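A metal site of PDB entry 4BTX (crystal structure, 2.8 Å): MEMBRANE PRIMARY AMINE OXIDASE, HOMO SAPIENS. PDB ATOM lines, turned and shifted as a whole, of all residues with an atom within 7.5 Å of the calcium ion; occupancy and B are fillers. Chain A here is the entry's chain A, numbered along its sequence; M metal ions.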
ATOM      1  N   GLU A 546      -7.327  15.350 -13.370  1.00  0.00           N
ATOM      2  CA  GLU A 546      -7.569  16.189 -14.541  1.00  0.00           C
ATOM      3  C   GLU A 546      -6.961  15.532 -15.802  1.00  0.00           C
ATOM      4  O   GLU A 546      -7.625  15.483 -16.847  1.00  0.00           O
ATOM      5  CB  GLU A 546      -7.109  17.655 -14.291  1.00  0.00           C
ATOM      6  CG  GLU A 546      -8.142  18.536 -13.563  1.00  0.00           C
ATOM      7  CD  GLU A 546      -7.692  19.974 -13.256  1.00  0.00           C
ATOM      8  OE1 GLU A 546      -6.502  20.191 -12.940  1.00  0.00           O
ATOM      9  OE2 GLU A 546      -8.532  20.910 -13.311  1.00  0.00           O
ATOM     10  N   VAL A 608     -11.506  17.845 -18.881  1.00  0.00           N
ATOM     11  CA  VAL A 608     -12.370  18.204 -17.767  1.00  0.00           C
ATOM     12  C   VAL A 608     -11.531  18.715 -16.630  1.00  0.00           C
ATOM     13  O   VAL A 608     -10.505  18.131 -16.281  1.00  0.00           O
ATOM     14  CB  VAL A 608     -13.252  17.049 -17.293  1.00  0.00           C
ATOM     15  CG1 VAL A 608     -13.990  17.479 -16.048  1.00  0.00           C
ATOM     16  CG2 VAL A 608     -14.261  16.671 -18.374  1.00  0.00           C
ATOM     17  N   THR A 609     -11.995  19.827 -16.082  1.00  0.00           N
ATOM     18  CA  THR A 609     -11.226  20.620 -15.181  1.00  0.00           C
ATOM     19  C   THR A 609     -12.127  21.044 -14.043  1.00  0.00           C
ATOM     20  O   THR A 609     -13.344  21.204 -14.226  1.00  0.00           O
ATOM     21  CB  THR A 609     -10.651  21.807 -15.982  1.00  0.00           C
ATOM     22  OG1 THR A 609      -9.321  21.469 -16.412  1.00  0.00           O
ATOM     23  CG2 THR A 609     -10.613  23.117 -15.183  1.00  0.00           C
ATOM     24  N   GLN A 610     -11.527  21.177 -12.855  1.00  0.00           N
ATOM     25  CA  GLN A 610     -12.129  21.924 -11.725  1.00  0.00           C
ATOM     26  C   GLN A 610     -12.509  23.333 -12.139  1.00  0.00           C
ATOM     27  O   GLN A 610     -11.609  24.098 -12.598  1.00  0.00           O
ATOM     28  CB  GLN A 610     -11.142  22.051 -10.565  1.00  0.00           C
ATOM     29  CG  GLN A 610     -11.221  20.939  -9.535  1.00  0.00           C
ATOM     30  CD  GLN A 610     -10.333  21.212  -8.333  1.00  0.00           C
ATOM     31  OE1 GLN A 610     -10.196  22.357  -7.905  1.00  0.00           O
ATOM     32  NE2 GLN A 610      -9.745  20.158  -7.774  1.00  0.00           N
ATOM     33  N   ARG A 611     -13.792  23.690 -11.964  1.00  0.00           N
ATOM     34  CA  ARG A 611     -14.316  25.031 -12.301  1.00  0.00           C
ATOM     35  C   ARG A 611     -13.699  26.057 -11.438  1.00  0.00           C
ATOM     36  O   ARG A 611     -13.397  25.765 -10.311  1.00  0.00           O
ATOM     37  CB  ARG A 611     -15.808  25.152 -12.067  1.00  0.00           C
ATOM     38  CG  ARG A 611     -16.488  25.932 -13.164  1.00  0.00           C
ATOM     39  CD  ARG A 611     -17.560  26.878 -12.676  1.00  0.00           C
ATOM     40  NE  ARG A 611     -16.995  28.063 -12.047  1.00  0.00           N
ATOM     41  CZ  ARG A 611     -17.516  29.294 -12.140  1.00  0.00           C
ATOM     42  NH1 ARG A 611     -18.601  29.547 -12.872  1.00  0.00           N
ATOM     43  NH2 ARG A 611     -16.923  30.293 -11.479  1.00  0.00           N
ATOM     44  N   LYS A 612     -13.535  27.284 -11.932  1.00  0.00           N
ATOM     45  CA  LYS A 612     -12.811  28.310 -11.152  1.00  0.00           C
ATOM     46  C   LYS A 612     -13.046  29.758 -11.557  1.00  0.00           C
ATOM     47  O   LYS A 612     -13.271  30.083 -12.743  1.00  0.00           O
ATOM     48  CB  LYS A 612     -11.318  28.050 -11.171  1.00  0.00           C
ATOM     49  CG  LYS A 612     -10.912  26.797 -10.433  1.00  0.00           C
ATOM     50  CD  LYS A 612      -9.423  26.765 -10.344  1.00  0.00           C
ATOM     51  CE  LYS A 612      -8.979  25.543  -9.581  1.00  0.00           C
ATOM     52  NZ  LYS A 612      -7.561  25.290  -9.928  1.00  0.00           N
ATOM     53  N   GLU A 615     -10.316  31.002 -13.722  1.00  0.00           N
ATOM     54  CA  GLU A 615     -10.245  30.352 -15.045  1.00  0.00           C
ATOM     55  C   GLU A 615     -11.599  30.524 -15.738  1.00  0.00           C
ATOM     56  O   GLU A 615     -12.268  29.564 -16.114  1.00  0.00           O
ATOM     57  CB  GLU A 615      -9.848  28.857 -14.913  1.00  0.00           C
ATOM     58  CG  GLU A 615      -8.458  28.628 -14.292  1.00  0.00           C
ATOM     59  CD  GLU A 615      -8.110  27.158 -13.972  1.00  0.00           C
ATOM     60  OE1 GLU A 615      -8.918  26.198 -14.145  1.00  0.00           O
ATOM     61  OE2 GLU A 615      -6.958  26.981 -13.521  1.00  0.00           O
ATOM     62  N   SER A 635      -3.816  25.241 -21.516  1.00  0.00           N
ATOM     63  CA  SER A 635      -3.163  24.050 -20.951  1.00  0.00           C
ATOM     64  C   SER A 635      -2.864  24.201 -19.464  1.00  0.00           C
ATOM     65  O   SER A 635      -2.657  23.205 -18.771  1.00  0.00           O
ATOM     66  CB  SER A 635      -1.874  23.729 -21.716  1.00  0.00           C
ATOM     67  OG  SER A 635      -0.842  24.616 -21.331  1.00  0.00           O
ATOM     68  N   ASP A 636      -2.842  25.430 -18.954  1.00  0.00           N
ATOM     69  CA  ASP A 636      -2.621  25.632 -17.519  1.00  0.00           C
ATOM     70  C   ASP A 636      -3.714  25.036 -16.634  1.00  0.00           C
ATOM     71  O   ASP A 636      -3.466  24.698 -15.468  1.00  0.00           O
ATOM     72  CB  ASP A 636      -2.471  27.115 -17.193  1.00  0.00           C
ATOM     73  CG  ASP A 636      -1.158  27.679 -17.636  1.00  0.00           C
ATOM     74  OD1 ASP A 636      -0.167  26.914 -17.701  1.00  0.00           O
ATOM     75  OD2 ASP A 636      -1.120  28.896 -17.929  1.00  0.00           O
ATOM     76  N   PHE A 637      -4.912  24.898 -17.190  1.00  0.00           N
ATOM     77  CA  PHE A 637      -6.074  24.458 -16.432  1.00  0.00           C
ATOM     78  C   PHE A 637      -5.954  22.983 -16.081  1.00  0.00           C
ATOM     79  O   PHE A 637      -6.592  22.477 -15.129  1.00  0.00           O
ATOM     80  CB  PHE A 637      -7.358  24.666 -17.246  1.00  0.00           C
ATOM     81  CG  PHE A 637      -7.641  26.104 -17.594  1.00  0.00           C
ATOM     82  CD1 PHE A 637      -6.716  27.125 -17.362  1.00  0.00           C
ATOM     83  CD2 PHE A 637      -8.853  26.442 -18.192  1.00  0.00           C
ATOM     84  CE1 PHE A 637      -6.993  28.421 -17.698  1.00  0.00           C
ATOM     85  CE2 PHE A 637      -9.138  27.736 -18.532  1.00  0.00           C
ATOM     86  CZ  PHE A 637      -8.202  28.730 -18.289  1.00  0.00           C
ATOM     87  N   ILE A 638      -5.141  22.273 -16.858  1.00  0.00           N
ATOM     88  CA  ILE A 638      -4.923  20.861 -16.653  1.00  0.00           C
ATOM     89  C   ILE A 638      -3.603  20.769 -15.926  1.00  0.00           C
ATOM     90  O   ILE A 638      -2.528  21.045 -16.486  1.00  0.00           O
ATOM     91  CB  ILE A 638      -4.964  20.115 -17.978  1.00  0.00           C
ATOM     92  CG1 ILE A 638      -6.297  20.383 -18.670  1.00  0.00           C
ATOM     93  CG2 ILE A 638      -4.809  18.632 -17.744  1.00  0.00           C
ATOM     94  CD1 ILE A 638      -6.261  20.214 -20.163  1.00  0.00           C
ATOM     95  N   ASN A 639      -3.712  20.432 -14.647  1.00  0.00           N
ATOM     96  CA  ASN A 639      -2.637  20.670 -13.683  1.00  0.00           C
ATOM     97  C   ASN A 639      -2.651  19.744 -12.500  1.00  0.00           C
ATOM     98  O   ASN A 639      -2.214  20.129 -11.430  1.00  0.00           O
ATOM     99  CB  ASN A 639      -2.680  22.134 -13.201  1.00  0.00           C
ATOM    100  CG  ASN A 639      -3.952  22.465 -12.407  1.00  0.00           C
ATOM    101  OD1 ASN A 639      -5.058  21.934 -12.644  1.00  0.00           O
ATOM    102  ND2 ASN A 639      -3.817  23.395 -11.474  1.00  0.00           N
ATOM    103  N   ASN A 640      -2.881  18.253 -12.820  1.00  0.00           N
ATOM    104  CA  ASN A 640      -3.421  17.177 -11.933  1.00  0.00           C
ATOM    105  C   ASN A 640      -3.965  17.626 -10.581  1.00  0.00           C
ATOM    106  O   ASN A 640      -3.258  17.739  -9.587  1.00  0.00           O
ATOM    107  CB  ASN A 640      -2.522  15.905 -11.831  1.00  0.00           C
ATOM    108  CG  ASN A 640      -1.223  16.119 -11.045  1.00  0.00           C
ATOM    109  OD1 ASN A 640      -0.154  15.659 -11.435  1.00  0.00           O
ATOM    110  ND2 ASN A 640      -1.326  16.857  -9.918  1.00  0.00           N
ATOM    111  N   GLU A 641      -5.077  17.767 -10.615  1.00  0.00           N
ATOM    112  CA  GLU A 641      -5.977  17.997  -9.502  1.00  0.00           C
ATOM    113  C   GLU A 641      -7.085  16.995  -9.591  1.00  0.00           C
ATOM    114  O   GLU A 641      -7.406  16.534 -10.677  1.00  0.00           O
ATOM    115  CB  GLU A 641      -6.620  19.361  -9.595  1.00  0.00           C
ATOM    116  CG  GLU A 641      -5.683  20.557  -9.602  1.00  0.00           C
ATOM    117  CD  GLU A 641      -6.435  21.865  -9.820  1.00  0.00           C
ATOM    118  OE1 GLU A 641      -7.203  21.965 -10.813  1.00  0.00           O
ATOM    119  OE2 GLU A 641      -6.283  22.788  -8.992  1.00  0.00           O
ATOM    120  N   THR A 642      -7.678  16.659  -8.459  1.00  0.00           N
ATOM    121  CA  THR A 642      -8.808  15.754  -8.455  1.00  0.00           C
ATOM    122  C   THR A 642     -10.005  16.357  -9.196  1.00  0.00           C
ATOM    123  O   THR A 642     -10.243  17.559  -9.204  1.00  0.00           O
ATOM    124  CB  THR A 642      -9.252  15.392  -7.022  1.00  0.00           C
ATOM    125  OG1 THR A 642     -10.350  14.473  -7.079  1.00  0.00           O
ATOM    126  CG2 THR A 642      -9.692  16.622  -6.247  1.00  0.00           C
ATOM    127  N   ILE A 643     -10.771  15.457  -9.807  1.00  0.00           N
ATOM    128  CA  ILE A 643     -12.066  15.777 -10.364  1.00  0.00           C
ATOM    129  C   ILE A 643     -13.083  14.778  -9.800  1.00  0.00           C
ATOM    130  O   ILE A 643     -14.180  14.570 -10.344  1.00  0.00           O
ATOM    131  CB  ILE A 643     -12.024  15.754 -11.898  1.00  0.00           C
ATOM    132  CG1 ILE A 643     -11.439  14.430 -12.429  1.00  0.00           C
ATOM    133  CG2 ILE A 643     -11.139  16.884 -12.388  1.00  0.00           C
ATOM    134  CD1 ILE A 643     -11.466  14.304 -13.930  1.00  0.00           C
HETATM  135 CA    CA M   1      -7.210  23.163 -12.892  1.00  0.00          CA
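The side-chain amino group (NZ) of Lys 612 lies within salt-bridge range of the side-chain carboxylate (OE2) of Glu 641 (3.0 Å).
The backbone carbonyl oxygen (O) of Phe 637 lies close to the side-chain hydroxyl (OG1) of Thr 609, at 3.2 Å.
The side-chain hydroxyl (OG1) of Thr 609 sits close to the side-chain carboxylate (OE2) of Glu 546, at 3.2 Å.
The side-chain carboxylate (OE2) of Glu 546 sits close to the backbone NH (N) of Gln 610, 3.0 Å away.
NZ of Lys 612 touches the calcium ion (3.7 Å).
Glu 615 touches the calcium ion (OE1 to CA, 3.7 Å).
Six residues have an atom within 4 Å of the calcium ion: Glu 546, Lys 612, Glu 615, Phe 637, Asn 639 and Glu 641.
The side-chain carboxylate (OE1) of Glu 641 binds the calcium ion (2.4 Å).
O of Phe 637 binds the calcium ion (2.4 Å).
OD1 of Asn 639 binds the calcium ion (2.5 Å).
OE2 of Glu 546 is bound to the calcium ion (2.6 Å).
The calcium ion has four donor atoms within binding distance.
Slightly farther from the calcium ion lies the side-chain carboxylate (OE1) of Glu 546 (3.1 Å).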
